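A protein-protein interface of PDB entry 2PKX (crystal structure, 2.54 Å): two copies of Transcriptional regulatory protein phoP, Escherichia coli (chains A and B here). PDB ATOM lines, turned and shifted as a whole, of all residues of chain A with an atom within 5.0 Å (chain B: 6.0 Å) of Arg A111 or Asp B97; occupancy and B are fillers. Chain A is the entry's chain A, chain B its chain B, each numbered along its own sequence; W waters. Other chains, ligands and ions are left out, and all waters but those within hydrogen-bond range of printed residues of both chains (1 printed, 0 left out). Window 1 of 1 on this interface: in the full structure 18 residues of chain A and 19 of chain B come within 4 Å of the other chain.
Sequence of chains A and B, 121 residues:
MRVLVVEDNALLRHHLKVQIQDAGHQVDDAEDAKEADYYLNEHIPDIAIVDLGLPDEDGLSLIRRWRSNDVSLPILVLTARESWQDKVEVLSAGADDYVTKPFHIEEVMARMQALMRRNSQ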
ATOM      1  N   LEU A  76      23.092  17.800  17.189  1.00  0.00           N
ATOM      2  CA  LEU A  76      22.256  18.937  17.429  1.00  0.00           C
ATOM      3  C   LEU A  76      23.040  20.094  16.833  1.00  0.00           C
ATOM      4  O   LEU A  76      24.200  20.352  17.190  1.00  0.00           O
ATOM      5  CB  LEU A  76      22.004  19.108  18.920  1.00  0.00           C
ATOM      6  CG  LEU A  76      21.293  20.388  19.440  1.00  0.00           C
ATOM      7  CD1 LEU A  76      19.862  20.496  18.955  1.00  0.00           C
ATOM      8  CD2 LEU A  76      21.321  20.500  20.952  1.00  0.00           C
ATOM      9  N   ASP A  97      18.484  17.730  15.295  1.00  0.00           N
ATOM     10  CA  ASP A  97      17.699  18.846  15.754  1.00  0.00           C
ATOM     11  C   ASP A  97      18.562  20.039  15.579  1.00  0.00           C
ATOM     12  O   ASP A  97      19.689  19.916  15.118  1.00  0.00           O
ATOM     13  CB  ASP A  97      17.270  18.674  17.240  1.00  0.00           C
ATOM     14  N   TYR A  98      18.037  21.196  15.942  1.00  0.00           N
ATOM     15  CA  TYR A  98      18.738  22.452  15.793  1.00  0.00           C
ATOM     16  C   TYR A  98      18.149  23.473  16.759  1.00  0.00           C
ATOM     17  O   TYR A  98      16.971  23.409  17.143  1.00  0.00           O
ATOM     18  CB  TYR A  98      18.631  22.977  14.360  1.00  0.00           C
ATOM     19  CG  TYR A  98      17.206  23.245  13.999  1.00  0.00           C
ATOM     20  CD1 TYR A  98      16.542  24.379  14.503  1.00  0.00           C
ATOM     21  CD2 TYR A  98      16.493  22.354  13.188  1.00  0.00           C
ATOM     22  CE1 TYR A  98      15.190  24.634  14.216  1.00  0.00           C
ATOM     23  CE2 TYR A  98      15.131  22.598  12.869  1.00  0.00           C
ATOM     24  CZ  TYR A  98      14.481  23.745  13.388  1.00  0.00           C
ATOM     25  OH  TYR A  98      13.137  23.998  13.096  1.00  0.00           O
ATOM     26  N   VAL A  99      18.993  24.405  17.167  1.00  0.00           N
ATOM     27  CA  VAL A  99      18.567  25.533  17.938  1.00  0.00           C
ATOM     28  C   VAL A  99      19.046  26.736  17.146  1.00  0.00           C
ATOM     29  O   VAL A  99      20.162  26.737  16.534  1.00  0.00           O
ATOM     30  CB  VAL A  99      19.170  25.551  19.312  1.00  0.00           C
ATOM     31  CG1 VAL A  99      18.489  26.615  20.140  1.00  0.00           C
ATOM     32  CG2 VAL A  99      18.977  24.203  19.999  1.00  0.00           C
ATOM     33  N   GLU A 107      17.589  25.852  26.667  1.00  0.00           N
ATOM     34  CA  GLU A 107      17.024  25.205  25.493  1.00  0.00           C
ATOM     35  C   GLU A 107      17.955  24.177  24.875  1.00  0.00           C
ATOM     36  O   GLU A 107      17.516  23.110  24.511  1.00  0.00           O
ATOM     37  CB  GLU A 107      16.618  26.190  24.412  1.00  0.00           C
ATOM     38  CG  GLU A 107      15.611  25.496  23.481  1.00  0.00           C
ATOM     39  CD  GLU A 107      15.081  26.364  22.384  1.00  0.00           C
ATOM     40  OE1 GLU A 107      14.952  27.588  22.630  1.00  0.00           O
ATOM     41  OE2 GLU A 107      14.785  25.817  21.283  1.00  0.00           O
ATOM     42  N   VAL A 108      19.226  24.523  24.758  1.00  0.00           N
ATOM     43  CA  VAL A 108      20.229  23.646  24.212  1.00  0.00           C
ATOM     44  C   VAL A 108      20.468  22.446  25.143  1.00  0.00           C
ATOM     45  O   VAL A 108      20.547  21.307  24.661  1.00  0.00           O
ATOM     46  CB  VAL A 108      21.533  24.438  23.919  1.00  0.00           C
ATOM     47  CG1 VAL A 108      22.710  23.487  23.523  1.00  0.00           C
ATOM     48  CG2 VAL A 108      21.289  25.548  22.833  1.00  0.00           C
ATOM     49  N   MET A 109      20.546  22.698  26.460  1.00  0.00           N
ATOM     50  CA  MET A 109      20.704  21.634  27.452  1.00  0.00           C
ATOM     51  C   MET A 109      19.529  20.676  27.327  1.00  0.00           C
ATOM     52  O   MET A 109      19.723  19.445  27.296  1.00  0.00           O
ATOM     53  CB  MET A 109      20.799  22.177  28.898  1.00  0.00           C
ATOM     54  CG  MET A 109      22.132  22.931  29.298  1.00  0.00           C
ATOM     55  SD  MET A 109      23.727  22.224  28.844  1.00  0.00           S
ATOM     56  CE  MET A 109      23.992  22.744  27.267  1.00  0.00           C
ATOM     57  N   ALA A 110      18.314  21.230  27.238  1.00  0.00           N
ATOM     58  CA  ALA A 110      17.125  20.408  27.095  1.00  0.00           C
ATOM     59  C   ALA A 110      17.064  19.560  25.804  1.00  0.00           C
ATOM     60  O   ALA A 110      16.537  18.441  25.822  1.00  0.00           O
ATOM     61  CB  ALA A 110      15.868  21.265  27.247  1.00  0.00           C
ATOM     62  N   ARG A 111      17.595  20.078  24.704  1.00  0.00           N
ATOM     63  CA  ARG A 111      17.630  19.333  23.430  1.00  0.00           C
ATOM     64  C   ARG A 111      18.664  18.218  23.476  1.00  0.00           C
ATOM     65  O   ARG A 111      18.401  17.116  22.995  1.00  0.00           O
ATOM     66  CB  ARG A 111      17.937  20.235  22.238  1.00  0.00           C
ATOM     67  CG  ARG A 111      16.989  21.408  21.955  1.00  0.00           C
ATOM     68  CD  ARG A 111      15.841  20.958  21.134  1.00  0.00           C
ATOM     69  NE  ARG A 111      15.422  21.890  20.081  1.00  0.00           N
ATOM     70  CZ  ARG A 111      14.443  21.597  19.228  1.00  0.00           C
ATOM     71  NH1 ARG A 111      13.810  20.421  19.348  1.00  0.00           N
ATOM     72  NH2 ARG A 111      14.085  22.460  18.274  1.00  0.00           N
ATOM     73  N   MET A 112      19.830  18.511  24.061  1.00  0.00           N
ATOM     74  CA  MET A 112      20.936  17.551  24.241  1.00  0.00           C
ATOM     75  C   MET A 112      20.439  16.379  25.122  1.00  0.00           C
ATOM     76  O   MET A 112      20.660  15.185  24.789  1.00  0.00           O
ATOM     77  CB  MET A 112      22.123  18.302  24.869  1.00  0.00           C
ATOM     78  CG  MET A 112      23.401  17.531  25.230  1.00  0.00           C
ATOM     79  SD  MET A 112      24.613  18.590  26.068  1.00  0.00           S
ATOM     80  CE  MET A 112      24.091  18.172  27.651  1.00  0.00           C
ATOM     81  N   GLN A 113      19.753  16.717  26.218  1.00  0.00           N
ATOM     82  CA  GLN A 113      19.217  15.709  27.119  1.00  0.00           C
ATOM     83  C   GLN A 113      18.168  14.877  26.422  1.00  0.00           C
ATOM     84  O   GLN A 113      18.257  13.649  26.463  1.00  0.00           O
ATOM     85  CB  GLN A 113      18.683  16.333  28.398  1.00  0.00           C
ATOM     86  CG  GLN A 113      19.797  16.370  29.470  1.00  0.00           C
ATOM     87  CD  GLN A 113      19.823  17.640  30.344  1.00  0.00           C
ATOM     88  OE1 GLN A 113      18.772  18.259  30.658  1.00  0.00           O
ATOM     89  NE2 GLN A 113      21.053  18.017  30.774  1.00  0.00           N
ATOM     90  N   ALA A 114      17.198  15.518  25.753  1.00  0.00           N
ATOM     91  CA  ALA A 114      16.217  14.766  24.990  1.00  0.00           C
ATOM     92  C   ALA A 114      16.913  13.720  24.115  1.00  0.00           C
ATOM     93  O   ALA A 114      16.490  12.569  24.099  1.00  0.00           O
ATOM     94  CB  ALA A 114      15.316  15.674  24.152  1.00  0.00           C
ATOM     95  N   LEU A 115      17.976  14.099  23.403  1.00  0.00           N
ATOM     96  CA  LEU A 115      18.659  13.145  22.543  1.00  0.00           C
ATOM     97  C   LEU A 115      19.464  12.064  23.283  1.00  0.00           C
ATOM     98  O   LEU A 115      19.449  10.906  22.889  1.00  0.00           O
ATOM     99  CB  LEU A 115      19.557  13.873  21.570  1.00  0.00           C
ATOM    100  CG  LEU A 115      18.836  14.563  20.421  1.00  0.00           C
ATOM    101  CD1 LEU A 115      19.813  15.459  19.727  1.00  0.00           C
ATOM    102  CD2 LEU A 115      18.284  13.529  19.482  1.00  0.00           C
ATOM    103  N   ILE B  75       8.154  10.867  20.461  1.00  0.00           N
ATOM    104  CA  ILE B  75       6.961  11.685  20.431  1.00  0.00           C
ATOM    105  C   ILE B  75       7.326  13.068  19.953  1.00  0.00           C
ATOM    106  O   ILE B  75       8.262  13.674  20.464  1.00  0.00           O
ATOM    107  CB  ILE B  75       6.289  11.758  21.823  1.00  0.00           C
ATOM    108  CG1 ILE B  75       6.022  10.324  22.375  1.00  0.00           C
ATOM    109  CG2 ILE B  75       5.029  12.693  21.774  1.00  0.00           C
ATOM    110  CD1 ILE B  75       5.550  10.228  23.801  1.00  0.00           C
ATOM    111  N   LEU B  76       6.615  13.539  18.936  1.00  0.00           N
ATOM    112  CA  LEU B  76       6.810  14.844  18.357  1.00  0.00           C
ATOM    113  C   LEU B  76       5.563  15.606  18.730  1.00  0.00           C
ATOM    114  O   LEU B  76       4.444  15.158  18.459  1.00  0.00           O
ATOM    115  CB  LEU B  76       6.887  14.715  16.851  1.00  0.00           C
ATOM    116  CG  LEU B  76       7.034  15.991  16.040  1.00  0.00           C
ATOM    117  CD1 LEU B  76       8.384  16.513  16.192  1.00  0.00           C
ATOM    118  CD2 LEU B  76       6.861  15.627  14.622  1.00  0.00           C
ATOM    119  N   VAL B  77       5.770  16.753  19.363  1.00  0.00           N
ATOM    120  CA  VAL B  77       4.680  17.535  19.907  1.00  0.00           C
ATOM    121  C   VAL B  77       4.255  18.640  18.933  1.00  0.00           C
ATOM    122  O   VAL B  77       5.078  19.257  18.254  1.00  0.00           O
ATOM    123  CB  VAL B  77       5.051  18.040  21.357  1.00  0.00           C
ATOM    124  CG1 VAL B  77       4.378  19.377  21.729  1.00  0.00           C
ATOM    125  CG2 VAL B  77       4.710  17.024  22.326  1.00  0.00           C
ATOM    126  N   LEU B  78       2.960  18.867  18.833  1.00  0.00           N
ATOM    127  CA  LEU B  78       2.480  20.042  18.119  1.00  0.00           C
ATOM    128  C   LEU B  78       1.990  20.968  19.212  1.00  0.00           C
ATOM    129  O   LEU B  78       1.284  20.537  20.140  1.00  0.00           O
ATOM    130  CB  LEU B  78       1.356  19.708  17.113  1.00  0.00           C
ATOM    131  CG  LEU B  78       1.571  18.609  16.057  1.00  0.00           C
ATOM    132  CD1 LEU B  78       0.321  18.401  15.168  1.00  0.00           C
ATOM    133  CD2 LEU B  78       2.792  18.869  15.195  1.00  0.00           C
ATOM    134  N   VAL B  90       8.162  20.977  27.768  1.00  0.00           N
ATOM    135  CA  VAL B  90       7.725  19.916  26.847  1.00  0.00           C
ATOM    136  C   VAL B  90       8.790  18.787  26.717  1.00  0.00           C
ATOM    137  O   VAL B  90       8.480  17.612  26.910  1.00  0.00           O
ATOM    138  CB  VAL B  90       7.361  20.501  25.441  1.00  0.00           C
ATOM    139  CG1 VAL B  90       7.078  19.415  24.463  1.00  0.00           C
ATOM    140  CG2 VAL B  90       6.124  21.402  25.536  1.00  0.00           C
ATOM    141  N   LEU B  91      10.036  19.157  26.402  1.00  0.00           N
ATOM    142  CA  LEU B  91      11.139  18.196  26.321  1.00  0.00           C
ATOM    143  C   LEU B  91      11.345  17.486  27.654  1.00  0.00           C
ATOM    144  O   LEU B  91      11.605  16.293  27.717  1.00  0.00           O
ATOM    145  CB  LEU B  91      12.421  18.871  25.873  1.00  0.00           C
ATOM    146  CG  LEU B  91      12.383  19.419  24.440  1.00  0.00           C
ATOM    147  CD1 LEU B  91      13.614  20.312  24.280  1.00  0.00           C
ATOM    148  CD2 LEU B  91      12.256  18.358  23.295  1.00  0.00           C
ATOM    149  N   ALA B  95       8.785  14.532  25.783  1.00  0.00           N
ATOM    150  CA  ALA B  95       8.780  14.664  24.326  1.00  0.00           C
ATOM    151  C   ALA B  95      10.201  14.730  23.794  1.00  0.00           C
ATOM    152  O   ALA B  95      11.149  15.213  24.462  1.00  0.00           O
ATOM    153  CB  ALA B  95       7.976  15.877  23.885  1.00  0.00           C
ATOM    154  N   ASP B  96      10.341  14.238  22.579  1.00  0.00           N
ATOM    155  CA  ASP B  96      11.590  14.240  21.893  1.00  0.00           C
ATOM    156  C   ASP B  96      11.739  15.483  21.044  1.00  0.00           C
ATOM    157  O   ASP B  96      12.843  15.870  20.701  1.00  0.00           O
ATOM    158  CB  ASP B  96      11.576  13.064  20.953  1.00  0.00           C
ATOM    159  CG  ASP B  96      11.743  11.786  21.662  1.00  0.00           C
ATOM    160  OD1 ASP B  96      12.905  11.437  21.901  1.00  0.00           O
ATOM    161  OD2 ASP B  96      10.731  11.140  21.994  1.00  0.00           O
ATOM    162  N   ASP B  97      10.624  16.100  20.665  1.00  0.00           N
ATOM    163  CA  ASP B  97      10.679  17.221  19.749  1.00  0.00           C
ATOM    164  C   ASP B  97       9.342  17.911  19.699  1.00  0.00           C
ATOM    165  O   ASP B  97       8.355  17.366  20.239  1.00  0.00           O
ATOM    166  CB  ASP B  97      11.106  16.721  18.369  1.00  0.00           C
ATOM    167  CG  ASP B  97      11.635  17.823  17.492  1.00  0.00           C
ATOM    168  OD1 ASP B  97      11.788  18.976  17.974  1.00  0.00           O
ATOM    169  OD2 ASP B  97      11.875  17.554  16.308  1.00  0.00           O
ATOM    170  N   TYR B  98       9.299  19.095  19.079  1.00  0.00           N
ATOM    171  CA  TYR B  98       8.072  19.884  18.977  1.00  0.00           C
ATOM    172  C   TYR B  98       8.047  20.703  17.713  1.00  0.00           C
ATOM    173  O   TYR B  98       9.089  21.089  17.201  1.00  0.00           O
ATOM    174  CB  TYR B  98       7.962  20.865  20.175  1.00  0.00           C
ATOM    175  CG  TYR B  98       9.217  21.637  20.359  1.00  0.00           C
ATOM    176  CD1 TYR B  98       9.550  22.663  19.484  1.00  0.00           C
ATOM    177  CD2 TYR B  98      10.096  21.308  21.378  1.00  0.00           C
ATOM    178  CE1 TYR B  98      10.761  23.371  19.615  1.00  0.00           C
ATOM    179  CE2 TYR B  98      11.303  21.986  21.539  1.00  0.00           C
ATOM    180  CZ  TYR B  98      11.639  23.021  20.652  1.00  0.00           C
ATOM    181  OH  TYR B  98      12.859  23.714  20.800  1.00  0.00           O
ATOM    182  N   VAL B  99       6.859  20.983  17.191  1.00  0.00           N
ATOM    183  CA  VAL B  99       6.741  22.033  16.171  1.00  0.00           C
ATOM    184  C   VAL B  99       5.753  23.070  16.628  1.00  0.00           C
ATOM    185  O   VAL B  99       4.697  22.740  17.147  1.00  0.00           O
ATOM    186  CB  VAL B  99       6.562  21.515  14.680  1.00  0.00           C
ATOM    187  CG1 VAL B  99       6.222  20.034  14.572  1.00  0.00           C
ATOM    188  CG2 VAL B  99       5.594  22.377  13.895  1.00  0.00           C
ATOM    189  N   ARG B 111      10.436  16.840  10.631  1.00  0.00           N
ATOM    190  CA  ARG B 111      10.749  16.423  12.006  1.00  0.00           C
ATOM    191  C   ARG B 111      10.493  14.918  12.299  1.00  0.00           C
ATOM    192  O   ARG B 111      11.304  14.277  12.981  1.00  0.00           O
ATOM    193  CB  ARG B 111       9.998  17.306  13.003  1.00  0.00           C
ATOM    194  CG  ARG B 111      10.822  18.428  13.625  1.00  0.00           C
ATOM    195  CD  ARG B 111      10.876  19.706  12.817  1.00  0.00           C
ATOM    196  NE  ARG B 111      10.907  20.906  13.672  1.00  0.00           N
ATOM    197  CZ  ARG B 111      11.790  21.143  14.661  1.00  0.00           C
ATOM    198  NH1 ARG B 111      12.748  20.251  14.979  1.00  0.00           N
ATOM    199  NH2 ARG B 111      11.711  22.290  15.358  1.00  0.00           N
ATOM    200  N   LEU B 115      13.123  11.799  13.321  1.00  0.00           N
ATOM    201  CA  LEU B 115      13.001  10.850  14.452  1.00  0.00           C
ATOM    202  C   LEU B 115      12.932   9.382  13.971  1.00  0.00           C
ATOM    203  O   LEU B 115      13.543   8.501  14.553  1.00  0.00           O
ATOM    204  CB  LEU B 115      11.803  11.181  15.343  1.00  0.00           C
ATOM    205  CG  LEU B 115      11.873  12.453  16.186  1.00  0.00           C
ATOM    206  CD1 LEU B 115      10.436  12.806  16.683  1.00  0.00           C
ATOM    207  CD2 LEU B 115      12.829  12.287  17.338  1.00  0.00           C
HETATM  208  O   HOH W   1      15.328  12.297  20.995  1.00  0.00           O
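Among the printed residues, merely in contact across the chains: Arg A111 with Arg B111, Ala A110 with Leu B91 and Arg A111 with Leu B91.
NH2 of Arg B111 is in hydrogen-bond range of OH of Tyr A98, at 3.2 Å.
OE2 of Glu A107 is in hydrogen-bond range of OH of Tyr B98, 2.9 Å away.
The guanidinium group (NH1) of Arg A111 is in salt-bridge range of the side-chain carboxylate (OD1) of Asp B97.
The guanidinium group (NH2) of Arg A111 lies within hydrogen-bond range of the side-chain hydroxyl (OH) of Tyr B98, 3.1 Å away.
Of the 13 printed residues of chain A, 4 touch a printed residue of chain B.
Hydrophobic or aromatic side chains of chain A that line the printed part of chain B: Tyr A98 and Ala A110.
Of the 13 printed residues of chain B, 4 touch a printed residue of chain A.
Printed residues of chain B that touch a printed residue of chain A: Leu B91, Asp B97, Tyr B98 and Arg B111.
Hydrophobic or aromatic side chains of chain B that line the printed part of chain A: Leu B91 and Tyr B98.
Water W1 lies within hydrogen-bond range of OD1 of Asp B96 (2.7 Å) and O of Ala A114 (3.3 Å).
NH2 of Arg A111 is in hydrogen-bond range of O of Tyr A98 (3.2 Å).
The backbone carbonyl oxygen of Ile B75 lies within hydrogen-bond range of the backbone NH of Asp B97 (3.4 Å).
The backbone NH (N) of Val B77 is in hydrogen-bond range of the backbone carbonyl oxygen (O) of Asp B97, 2.8 Å away.
The side-chain carboxylate of Asp B97 lies within salt-bridge range of the guanidinium group of Arg B111 (3.1 Å).
The backbone carbonyl oxygen of Tyr B98 lies within hydrogen-bond range of the guanidinium group of Arg B111 (3.4 Å).
Of the printed residues of chain B, Tyr A98 touches Arg B111.
Of the printed residues of chain B, Glu A107 touches Tyr B98.
Of chain B, only Leu B91, Asp B97, Tyr B98 and Arg B111 come within 4 Å of Arg A111.
Val B77 touches none of the printed residues of chain A.
Of chain A, only Arg A111 comes within 4 Å of Asp B97.
Of the printed residues of chain A, Tyr B98 touches Glu A107 and Arg A111.
Of the printed residues of chain A, Arg B111 touches Tyr A98 (3.2 Å) and Arg A111 (3.8 Å).
The nearest printed residue of chain A that does not touch Asp B97 is Asp A97 (5.5 Å).
Tyr A98 touches Arg B111, and with the chains exchanged Arg A111 touches Tyr B98.
Arg A111 touches Asp B97, but with the chains exchanged Asp A97 does not touch Arg B111 (5.2 Å).
Arg A111 touches its own counterpart, Arg B111.
Positions printed for both chains: 76, 97, 98, 99, 111 and 115.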
